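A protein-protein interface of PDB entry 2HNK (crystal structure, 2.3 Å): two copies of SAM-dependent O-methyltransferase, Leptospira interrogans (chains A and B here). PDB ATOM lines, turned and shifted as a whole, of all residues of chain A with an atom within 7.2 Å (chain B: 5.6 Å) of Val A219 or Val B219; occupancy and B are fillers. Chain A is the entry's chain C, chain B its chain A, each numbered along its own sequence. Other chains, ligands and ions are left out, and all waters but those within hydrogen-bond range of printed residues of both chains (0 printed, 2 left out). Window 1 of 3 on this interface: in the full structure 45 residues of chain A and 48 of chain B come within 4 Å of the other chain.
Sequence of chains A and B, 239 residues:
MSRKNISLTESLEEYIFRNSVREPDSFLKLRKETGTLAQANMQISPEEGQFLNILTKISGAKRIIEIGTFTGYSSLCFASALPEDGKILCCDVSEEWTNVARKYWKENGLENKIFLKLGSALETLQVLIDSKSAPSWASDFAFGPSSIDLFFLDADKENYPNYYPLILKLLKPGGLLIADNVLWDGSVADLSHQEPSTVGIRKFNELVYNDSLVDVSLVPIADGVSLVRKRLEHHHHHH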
ATOM      1  N   ASN A   5     -32.172  24.599  14.207  1.00  0.00           N
ATOM      2  CA  ASN A   5     -32.710  25.177  15.425  1.00  0.00           C
ATOM      3  C   ASN A   5     -34.039  25.844  15.170  1.00  0.00           C
ATOM      4  O   ASN A   5     -34.264  26.421  14.106  1.00  0.00           O
ATOM      5  CB  ASN A   5     -31.728  26.182  16.025  1.00  0.00           C
ATOM      6  CG  ASN A   5     -30.373  25.571  16.300  1.00  0.00           C
ATOM      7  OD1 ASN A   5     -30.182  24.885  17.304  1.00  0.00           O
ATOM      8  ND2 ASN A   5     -29.418  25.813  15.401  1.00  0.00           N
ATOM      9  N   ILE A   6     -34.913  25.750  16.166  1.00  0.00           N
ATOM     10  CA  ILE A   6     -36.224  26.361  16.149  1.00  0.00           C
ATOM     11  C   ILE A   6     -36.153  27.856  15.808  1.00  0.00           C
ATOM     12  O   ILE A   6     -35.274  28.569  16.286  1.00  0.00           O
ATOM     13  CB  ILE A   6     -36.941  26.133  17.514  1.00  0.00           C
ATOM     14  CG1 ILE A   6     -38.411  26.581  17.458  1.00  0.00           C
ATOM     15  CG2 ILE A   6     -36.162  26.792  18.676  1.00  0.00           C
ATOM     16  CD1 ILE A   6     -39.278  25.975  18.529  1.00  0.00           C
ATOM     17  N   ILE A  16     -40.598  31.277  26.828  1.00  0.00           N
ATOM     18  CA  ILE A  16     -39.316  30.845  27.413  1.00  0.00           C
ATOM     19  C   ILE A  16     -39.035  31.564  28.739  1.00  0.00           C
ATOM     20  O   ILE A  16     -38.798  30.923  29.763  1.00  0.00           O
ATOM     21  CB  ILE A  16     -38.123  31.027  26.430  1.00  0.00           C
ATOM     22  CG1 ILE A  16     -38.272  30.092  25.223  1.00  0.00           C
ATOM     23  CG2 ILE A  16     -36.811  30.752  27.132  1.00  0.00           C
ATOM     24  CD1 ILE A  16     -37.369  30.426  24.041  1.00  0.00           C
ATOM     25  N   SER A  20     -38.823  29.753  32.548  1.00  0.00           N
ATOM     26  CA  SER A  20     -37.445  29.428  32.928  1.00  0.00           C
ATOM     27  C   SER A  20     -36.790  30.476  33.813  1.00  0.00           C
ATOM     28  O   SER A  20     -35.870  30.165  34.569  1.00  0.00           O
ATOM     29  CB  SER A  20     -36.578  29.177  31.691  1.00  0.00           C
ATOM     30  OG  SER A  20     -36.438  30.361  30.923  1.00  0.00           O
ATOM     31  N   GLU A  47     -32.162  35.123  30.562  1.00  0.00           N
ATOM     32  CA  GLU A  47     -32.064  33.751  30.075  1.00  0.00           C
ATOM     33  C   GLU A  47     -30.609  33.291  30.029  1.00  0.00           C
ATOM     34  O   GLU A  47     -30.273  32.220  30.526  1.00  0.00           O
ATOM     35  CB  GLU A  47     -32.687  33.618  28.679  1.00  0.00           C
ATOM     36  CG  GLU A  47     -34.213  33.765  28.599  1.00  0.00           C
ATOM     37  CD  GLU A  47     -34.693  35.212  28.545  1.00  0.00           C
ATOM     38  OE1 GLU A  47     -35.929  35.415  28.501  1.00  0.00           O
ATOM     39  OE2 GLU A  47     -33.850  36.142  28.550  1.00  0.00           O
ATOM     40  N   PHE A  51     -28.580  30.425  32.254  1.00  0.00           N
ATOM     41  CA  PHE A  51     -27.719  29.463  31.593  1.00  0.00           C
ATOM     42  C   PHE A  51     -26.354  29.406  32.286  1.00  0.00           C
ATOM     43  O   PHE A  51     -25.860  28.326  32.599  1.00  0.00           O
ATOM     44  CB  PHE A  51     -27.607  29.836  30.110  1.00  0.00           C
ATOM     45  CG  PHE A  51     -26.830  28.850  29.271  1.00  0.00           C
ATOM     46  CD1 PHE A  51     -27.199  27.505  29.213  1.00  0.00           C
ATOM     47  CD2 PHE A  51     -25.753  29.285  28.499  1.00  0.00           C
ATOM     48  CE1 PHE A  51     -26.496  26.610  28.427  1.00  0.00           C
ATOM     49  CE2 PHE A  51     -25.042  28.390  27.709  1.00  0.00           C
ATOM     50  CZ  PHE A  51     -25.419  27.048  27.674  1.00  0.00           C
ATOM     51  N   ILE A  54     -26.858  27.759  35.846  1.00  0.00           N
ATOM     52  CA  ILE A  54     -26.939  26.298  35.837  1.00  0.00           C
ATOM     53  C   ILE A  54     -25.596  25.638  35.498  1.00  0.00           C
ATOM     54  O   ILE A  54     -25.201  24.653  36.127  1.00  0.00           O
ATOM     55  CB  ILE A  54     -28.117  25.765  34.949  1.00  0.00           C
ATOM     56  CG1 ILE A  54     -28.572  24.386  35.421  1.00  0.00           C
ATOM     57  CG2 ILE A  54     -27.763  25.710  33.463  1.00  0.00           C
ATOM     58  CD1 ILE A  54     -29.893  24.401  36.131  1.00  0.00           C
ATOM     59  N   LEU A  55     -24.892  26.199  34.519  1.00  0.00           N
ATOM     60  CA  LEU A  55     -23.576  25.702  34.128  1.00  0.00           C
ATOM     61  C   LEU A  55     -22.564  25.763  35.267  1.00  0.00           C
ATOM     62  O   LEU A  55     -21.751  24.861  35.422  1.00  0.00           O
ATOM     63  CB  LEU A  55     -23.047  26.482  32.928  1.00  0.00           C
ATOM     64  CG  LEU A  55     -22.997  25.884  31.515  1.00  0.00           C
ATOM     65  CD1 LEU A  55     -23.947  24.720  31.251  1.00  0.00           C
ATOM     66  CD2 LEU A  55     -23.187  27.006  30.478  1.00  0.00           C
ATOM     67  N   ALA A 179     -17.509  31.363  26.444  1.00  0.00           N
ATOM     68  CA  ALA A 179     -17.196  32.527  25.626  1.00  0.00           C
ATOM     69  C   ALA A 179     -18.445  33.188  25.060  1.00  0.00           C
ATOM     70  O   ALA A 179     -19.260  32.544  24.394  1.00  0.00           O
ATOM     71  CB  ALA A 179     -16.209  32.154  24.509  1.00  0.00           C
ATOM     72  N   VAL A 182     -19.859  34.970  20.395  1.00  0.00           N
ATOM     73  CA  VAL A 182     -19.114  34.205  19.393  1.00  0.00           C
ATOM     74  C   VAL A 182     -19.742  34.239  17.993  1.00  0.00           C
ATOM     75  O   VAL A 182     -19.111  33.839  17.017  1.00  0.00           O
ATOM     76  CB  VAL A 182     -18.819  32.736  19.853  1.00  0.00           C
ATOM     77  CG1 VAL A 182     -17.828  32.717  21.031  1.00  0.00           C
ATOM     78  CG2 VAL A 182     -20.102  31.972  20.197  1.00  0.00           C
ATOM     79  N   LEU A 183     -20.971  34.734  17.895  1.00  0.00           N
ATOM     80  CA  LEU A 183     -21.627  34.881  16.591  1.00  0.00           C
ATOM     81  C   LEU A 183     -21.639  36.334  16.100  1.00  0.00           C
ATOM     82  O   LEU A 183     -21.881  36.587  14.926  1.00  0.00           O
ATOM     83  CB  LEU A 183     -23.030  34.266  16.604  1.00  0.00           C
ATOM     84  CG  LEU A 183     -23.056  32.735  16.771  1.00  0.00           C
ATOM     85  CD1 LEU A 183     -24.472  32.214  16.856  1.00  0.00           C
ATOM     86  CD2 LEU A 183     -22.287  32.030  15.650  1.00  0.00           C
ATOM     87  N   VAL A 216     -15.557  21.727  22.012  1.00  0.00           N
ATOM     88  CA  VAL A 216     -16.403  22.913  21.888  1.00  0.00           C
ATOM     89  C   VAL A 216     -17.865  22.594  21.547  1.00  0.00           C
ATOM     90  O   VAL A 216     -18.157  21.735  20.716  1.00  0.00           O
ATOM     91  CB  VAL A 216     -15.792  23.957  20.881  1.00  0.00           C
ATOM     92  CG1 VAL A 216     -15.494  23.321  19.526  1.00  0.00           C
ATOM     93  CG2 VAL A 216     -16.681  25.204  20.734  1.00  0.00           C
ATOM     94  N   SER A 217     -18.768  23.307  22.211  1.00  0.00           N
ATOM     95  CA  SER A 217     -20.163  23.352  21.812  1.00  0.00           C
ATOM     96  C   SER A 217     -20.570  24.813  21.658  1.00  0.00           C
ATOM     97  O   SER A 217     -20.502  25.583  22.615  1.00  0.00           O
ATOM     98  CB  SER A 217     -21.054  22.638  22.828  1.00  0.00           C
ATOM     99  OG  SER A 217     -22.411  22.701  22.421  1.00  0.00           O
ATOM    100  N   LEU A 218     -20.965  25.189  20.444  1.00  0.00           N
ATOM    101  CA  LEU A 218     -21.354  26.560  20.141  1.00  0.00           C
ATOM    102  C   LEU A 218     -22.883  26.690  20.146  1.00  0.00           C
ATOM    103  O   LEU A 218     -23.569  26.308  19.194  1.00  0.00           O
ATOM    104  CB  LEU A 218     -20.761  27.007  18.801  1.00  0.00           C
ATOM    105  CG  LEU A 218     -20.633  28.521  18.542  1.00  0.00           C
ATOM    106  CD1 LEU A 218     -19.780  28.777  17.302  1.00  0.00           C
ATOM    107  CD2 LEU A 218     -21.992  29.235  18.435  1.00  0.00           C
ATOM    108  N   VAL A 219     -23.389  27.259  21.232  1.00  0.00           N
ATOM    109  CA  VAL A 219     -24.808  27.263  21.543  1.00  0.00           C
ATOM    110  C   VAL A 219     -25.434  28.547  21.004  1.00  0.00           C
ATOM    111  O   VAL A 219     -24.965  29.633  21.325  1.00  0.00           O
ATOM    112  CB  VAL A 219     -25.008  27.182  23.084  1.00  0.00           C
ATOM    113  CG1 VAL A 219     -26.482  27.104  23.450  1.00  0.00           C
ATOM    114  CG2 VAL A 219     -24.240  26.004  23.660  1.00  0.00           C
ATOM    115  N   PRO A 220     -26.492  28.431  20.174  1.00  0.00           N
ATOM    116  CA  PRO A 220     -27.098  29.658  19.646  1.00  0.00           C
ATOM    117  C   PRO A 220     -28.028  30.356  20.644  1.00  0.00           C
ATOM    118  O   PRO A 220     -29.178  30.679  20.331  1.00  0.00           O
ATOM    119  CB  PRO A 220     -27.833  29.179  18.390  1.00  0.00           C
ATOM    120  CG  PRO A 220     -28.190  27.747  18.682  1.00  0.00           C
ATOM    121  CD  PRO A 220     -27.146  27.215  19.647  1.00  0.00           C
ATOM    122  N   ILE A 221     -27.520  30.591  21.846  1.00  0.00           N
ATOM    123  CA  ILE A 221     -28.242  31.383  22.825  1.00  0.00           C
ATOM    124  C   ILE A 221     -27.639  32.793  22.837  1.00  0.00           C
ATOM    125  O   ILE A 221     -26.422  32.958  22.667  1.00  0.00           O
ATOM    126  CB  ILE A 221     -28.258  30.709  24.240  1.00  0.00           C
ATOM    127  CG1 ILE A 221     -29.202  31.457  25.196  1.00  0.00           C
ATOM    128  CG2 ILE A 221     -26.846  30.585  24.817  1.00  0.00           C
ATOM    129  CD1 ILE A 221     -29.299  30.845  26.589  1.00  0.00           C
ATOM    130  N   ALA A 222     -28.493  33.797  23.015  1.00  0.00           N
ATOM    131  CA  ALA A 222     -28.085  35.205  22.972  1.00  0.00           C
ATOM    132  C   ALA A 222     -27.354  35.520  21.657  1.00  0.00           C
ATOM    133  O   ALA A 222     -27.920  35.326  20.585  1.00  0.00           O
ATOM    134  CB  ALA A 222     -27.251  35.571  24.194  1.00  0.00           C
ATOM    135  N   ASP A 223     -26.108  35.983  21.741  1.00  0.00           N
ATOM    136  CA  ASP A 223     -25.309  36.313  20.557  1.00  0.00           C
ATOM    137  C   ASP A 223     -24.278  35.216  20.249  1.00  0.00           C
ATOM    138  O   ASP A 223     -23.194  35.488  19.708  1.00  0.00           O
ATOM    139  CB  ASP A 223     -24.622  37.669  20.770  1.00  0.00           C
ATOM    140  CG  ASP A 223     -24.001  38.229  19.497  1.00  0.00           C
ATOM    141  OD1 ASP A 223     -24.590  38.074  18.404  1.00  0.00           O
ATOM    142  OD2 ASP A 223     -22.914  38.821  19.602  1.00  0.00           O
ATOM    143  N   GLY A 224     -24.629  33.975  20.594  1.00  0.00           N
ATOM    144  CA  GLY A 224     -23.724  32.834  20.500  1.00  0.00           C
ATOM    145  C   GLY A 224     -22.951  32.679  21.794  1.00  0.00           C
ATOM    146  O   GLY A 224     -22.376  33.640  22.305  1.00  0.00           O
ATOM    147  N   VAL A 225     -22.967  31.470  22.348  1.00  0.00           N
ATOM    148  CA  VAL A 225     -22.178  31.166  23.542  1.00  0.00           C
ATOM    149  C   VAL A 225     -21.441  29.844  23.326  1.00  0.00           C
ATOM    150  O   VAL A 225     -22.073  28.800  23.118  1.00  0.00           O
ATOM    151  CB  VAL A 225     -23.045  31.098  24.830  1.00  0.00           C
ATOM    152  CG1 VAL A 225     -22.171  30.811  26.033  1.00  0.00           C
ATOM    153  CG2 VAL A 225     -23.823  32.401  25.059  1.00  0.00           C
ATOM    154  N   SER A 226     -20.110  29.900  23.357  1.00  0.00           N
ATOM    155  CA  SER A 226     -19.291  28.710  23.195  1.00  0.00           C
ATOM    156  C   SER A 226     -18.938  28.113  24.523  1.00  0.00           C
ATOM    157  O   SER A 226     -18.461  28.806  25.422  1.00  0.00           O
ATOM    158  CB  SER A 226     -18.010  29.002  22.416  1.00  0.00           C
ATOM    159  OG  SER A 226     -18.276  29.003  21.033  1.00  0.00           O
ATOM    160  N   LEU A 227     -19.187  26.816  24.638  1.00  0.00           N
ATOM    161  CA  LEU A 227     -18.772  26.048  25.798  1.00  0.00           C
ATOM    162  C   LEU A 227     -17.504  25.331  25.389  1.00  0.00           C
ATOM    163  O   LEU A 227     -17.535  24.451  24.527  1.00  0.00           O
ATOM    164  CB  LEU A 227     -19.871  25.062  26.202  1.00  0.00           C
ATOM    165  CG  LEU A 227     -21.225  25.708  26.545  1.00  0.00           C
ATOM    166  CD1 LEU A 227     -22.249  24.666  26.947  1.00  0.00           C
ATOM    167  CD2 LEU A 227     -21.069  26.781  27.636  1.00  0.00           C
ATOM    168  N   PHE B  51     -23.310  19.086  22.165  1.00  0.00           N
ATOM    169  CA  PHE B  51     -23.797  19.794  23.341  1.00  0.00           C
ATOM    170  C   PHE B  51     -24.013  18.799  24.497  1.00  0.00           C
ATOM    171  O   PHE B  51     -23.608  19.054  25.630  1.00  0.00           O
ATOM    172  CB  PHE B  51     -25.100  20.523  22.993  1.00  0.00           C
ATOM    173  CG  PHE B  51     -25.696  21.317  24.134  1.00  0.00           C
ATOM    174  CD1 PHE B  51     -24.950  22.285  24.804  1.00  0.00           C
ATOM    175  CD2 PHE B  51     -27.012  21.125  24.506  1.00  0.00           C
ATOM    176  CE1 PHE B  51     -25.509  23.036  25.832  1.00  0.00           C
ATOM    177  CE2 PHE B  51     -27.585  21.879  25.533  1.00  0.00           C
ATOM    178  CZ  PHE B  51     -26.829  22.842  26.193  1.00  0.00           C
ATOM    179  N   VAL B 182     -38.630  20.682  24.328  1.00  0.00           N
ATOM    180  CA  VAL B 182     -39.420  21.462  25.292  1.00  0.00           C
ATOM    181  C   VAL B 182     -40.138  22.673  24.672  1.00  0.00           C
ATOM    182  O   VAL B 182     -41.030  23.251  25.289  1.00  0.00           O
ATOM    183  CB  VAL B 182     -38.613  21.851  26.561  1.00  0.00           C
ATOM    184  CG1 VAL B 182     -38.332  20.609  27.423  1.00  0.00           C
ATOM    185  CG2 VAL B 182     -37.311  22.590  26.207  1.00  0.00           C
ATOM    186  N   LEU B 183     -39.762  23.030  23.447  1.00  0.00           N
ATOM    187  CA  LEU B 183     -40.450  24.080  22.709  1.00  0.00           C
ATOM    188  C   LEU B 183     -41.432  23.515  21.681  1.00  0.00           C
ATOM    189  O   LEU B 183     -42.332  24.217  21.242  1.00  0.00           O
ATOM    190  CB  LEU B 183     -39.454  25.092  22.099  1.00  0.00           C
ATOM    191  CG  LEU B 183     -38.701  25.930  23.150  1.00  0.00           C
ATOM    192  CD1 LEU B 183     -37.643  26.833  22.537  1.00  0.00           C
ATOM    193  CD2 LEU B 183     -39.661  26.739  24.037  1.00  0.00           C
ATOM    194  N   SER B 217     -32.723  25.858  33.073  1.00  0.00           N
ATOM    195  CA  SER B 217     -32.323  26.727  31.980  1.00  0.00           C
ATOM    196  C   SER B 217     -32.909  26.121  30.707  1.00  0.00           C
ATOM    197  O   SER B 217     -32.635  24.970  30.386  1.00  0.00           O
ATOM    198  CB  SER B 217     -30.795  26.821  31.870  1.00  0.00           C
ATOM    199  OG  SER B 217     -30.406  27.640  30.769  1.00  0.00           O
ATOM    200  N   LEU B 218     -33.737  26.890  30.007  1.00  0.00           N
ATOM    201  CA  LEU B 218     -34.368  26.428  28.780  1.00  0.00           C
ATOM    202  C   LEU B 218     -33.618  27.042  27.608  1.00  0.00           C
ATOM    203  O   LEU B 218     -33.753  28.239  27.319  1.00  0.00           O
ATOM    204  CB  LEU B 218     -35.862  26.789  28.752  1.00  0.00           C
ATOM    205  CG  LEU B 218     -36.811  26.035  27.798  1.00  0.00           C
ATOM    206  CD1 LEU B 218     -38.267  26.326  28.120  1.00  0.00           C
ATOM    207  CD2 LEU B 218     -36.525  26.328  26.326  1.00  0.00           C
ATOM    208  N   VAL B 219     -32.830  26.199  26.944  1.00  0.00           N
ATOM    209  CA  VAL B 219     -31.899  26.612  25.904  1.00  0.00           C
ATOM    210  C   VAL B 219     -32.557  26.468  24.522  1.00  0.00           C
ATOM    211  O   VAL B 219     -33.039  25.391  24.177  1.00  0.00           O
ATOM    212  CB  VAL B 219     -30.565  25.786  25.991  1.00  0.00           C
ATOM    213  CG1 VAL B 219     -29.540  26.293  25.003  1.00  0.00           C
ATOM    214  CG2 VAL B 219     -29.985  25.839  27.407  1.00  0.00           C
ATOM    215  N   PRO B 220     -32.590  27.560  23.732  1.00  0.00           N
ATOM    216  CA  PRO B 220     -33.169  27.488  22.381  1.00  0.00           C
ATOM    217  C   PRO B 220     -32.271  26.823  21.332  1.00  0.00           C
ATOM    218  O   PRO B 220     -32.102  27.347  20.238  1.00  0.00           O
ATOM    219  CB  PRO B 220     -33.453  28.956  22.029  1.00  0.00           C
ATOM    220  CG  PRO B 220     -32.531  29.745  22.865  1.00  0.00           C
ATOM    221  CD  PRO B 220     -32.127  28.920  24.069  1.00  0.00           C
ATOM    222  N   ILE B 221     -31.711  25.667  21.658  1.00  0.00           N
ATOM    223  CA  ILE B 221     -30.998  24.867  20.676  1.00  0.00           C
ATOM    224  C   ILE B 221     -31.944  23.754  20.216  1.00  0.00           C
ATOM    225  O   ILE B 221     -32.782  23.283  21.000  1.00  0.00           O
ATOM    226  CB  ILE B 221     -29.641  24.317  21.238  1.00  0.00           C
ATOM    227  CG1 ILE B 221     -28.834  23.587  20.150  1.00  0.00           C
ATOM    228  CG2 ILE B 221     -29.854  23.438  22.478  1.00  0.00           C
ATOM    229  CD1 ILE B 221     -27.348  23.395  20.495  1.00  0.00           C
ATOM    230  N   GLY B 224     -35.629  23.120  21.442  1.00  0.00           N
ATOM    231  CA  GLY B 224     -35.672  23.477  22.847  1.00  0.00           C
ATOM    232  C   GLY B 224     -35.079  22.348  23.664  1.00  0.00           C
ATOM    233  O   GLY B 224     -35.466  21.183  23.505  1.00  0.00           O
ATOM    234  N   VAL B 225     -34.110  22.692  24.511  1.00  0.00           N
ATOM    235  CA  VAL B 225     -33.501  21.746  25.438  1.00  0.00           C
ATOM    236  C   VAL B 225     -33.506  22.386  26.818  1.00  0.00           C
ATOM    237  O   VAL B 225     -32.942  23.465  27.011  1.00  0.00           O
ATOM    238  CB  VAL B 225     -32.039  21.380  25.051  1.00  0.00           C
ATOM    239  CG1 VAL B 225     -31.429  20.405  26.064  1.00  0.00           C
ATOM    240  CG2 VAL B 225     -31.968  20.775  23.647  1.00  0.00           C
ATOM    241  N   SER B 226     -34.153  21.728  27.776  1.00  0.00           N
ATOM    242  CA  SER B 226     -34.110  22.193  29.154  1.00  0.00           C
ATOM    243  C   SER B 226     -33.033  21.469  29.949  1.00  0.00           C
ATOM    244  O   SER B 226     -32.947  20.234  29.933  1.00  0.00           O
ATOM    245  CB  SER B 226     -35.469  22.053  29.842  1.00  0.00           C
ATOM    246  OG  SER B 226     -36.286  23.162  29.534  1.00  0.00           O
ATOM    247  N   LEU B 227     -32.204  22.262  30.619  1.00  0.00           N
ATOM    248  CA  LEU B 227     -31.283  21.746  31.623  1.00  0.00           C
ATOM    249  C   LEU B 227     -31.959  21.917  32.979  1.00  0.00           C
ATOM    250  O   LEU B 227     -32.245  23.036  33.392  1.00  0.00           O
ATOM    251  CB  LEU B 227     -29.940  22.475  31.575  1.00  0.00           C
ATOM    252  CG  LEU B 227     -29.257  22.511  30.205  1.00  0.00           C
ATOM    253  CD1 LEU B 227     -27.911  23.245  30.277  1.00  0.00           C
ATOM    254  CD2 LEU B 227     -29.117  21.098  29.633  1.00  0.00           C
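Among the printed residues, merely in contact across the chains: Ser A217 with Phe B51, Phe A51 with Ser B217, Asn A5 with Ile B221, Val A219 with Val B219, Ile A54 with Ser B217, Ile A6 with Leu B183, Phe A51 with Val B219, Leu A227 with Phe B51, Ile A16 with Leu B183, Ser A20 with Leu B218, Ile A54 with Leu B227, Val A219 with Phe B51, Pro A220 with Ile B221 and Ile A16 with Leu B218.
Of chain B, only Phe B51 and Val B219 come within 4 Å of Val A219.
Val B219 touches two residues of chain A.
Of the printed residues of chain B, Phe A51 touches Ser B217 (3.3 Å) and Val B219 (3.7 Å).
Of the printed residues of chain A, Leu B218 touches Ile A16 and Ser A20.
Printed residues of chain A within 4 Å of Leu B227: Ile A54.
Of the printed residues of chain A, Ile B221 touches Asn A5 (3.4 Å) and Pro A220 (3.9 Å).
Of the printed residues of chain A, Leu B183 touches Ile A6 and Ile A16.
Leu A183 touches none of the printed residues of chain B.
The nearest residue of chain A that does not touch Val B219 is Ile A221 (4.7 Å).
Phe A51 touches Ser B217, and with the chains exchanged Ser A217 touches Phe B51.
Val B219 touches its own counterpart, Val A219.
Pro A220 touches Ile B221, but with the chains exchanged Ile A221 does not touch Pro B220 (4.03 Å).
Leu A227 touches Phe B51, but with the chains exchanged Phe A51 does not touch Leu B227 (4.1 Å).
12 positions are printed for both chains.
Of the 14 pairs that touch across the chains among the printed residues, 5 have their exchanged pair printed and touching as well.
The backbone carbonyl oxygen (O) of Ser B217 is in hydrogen-bond range of the backbone NH (N) of Leu B227, 2.8 Å away.
OG of Ser A20 is in hydrogen-bond range of O of Ile A16 (2.7 Å).
The backbone NH of Val A219 sits at hydrogen-bond distance from the backbone carbonyl oxygen of Val A225, 2.8 Å away.
The backbone NH (N) of Leu A227 sits at hydrogen-bond distance from the backbone carbonyl oxygen (O) of Ser A217, at 2.7 Å.
The backbone carbonyl oxygen (O) of Val B225 lies within hydrogen-bond range of the backbone NH (N) of Val B219, 2.7 Å away.
Printed residues of chain A that touch a printed residue of chain B: Asn A5, Ile A6, Ile A16, Ser A20, Phe A51, Ile A54, Ser A217, Val A219, Pro A220 and Leu A227.
Hydrophobic or aromatic side chains of chain A that line the printed part of chain B: Ile A6, Ile A16, Phe A51, Ile A54, Val A219, Pro A220 and Leu A227.
Of the 12 printed residues of chain B, 7 touch a printed residue of chain A.
Printed residues of chain B that touch a printed residue of chain A: Phe B51, Leu B183, Ser B217, Leu B218, Val B219, Ile B221 and Leu B227.
Hydrophobic or aromatic side chains of chain B that line the printed part of chain A: Phe B51, Leu B183, Leu B218, Val B219 and Ile B221.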
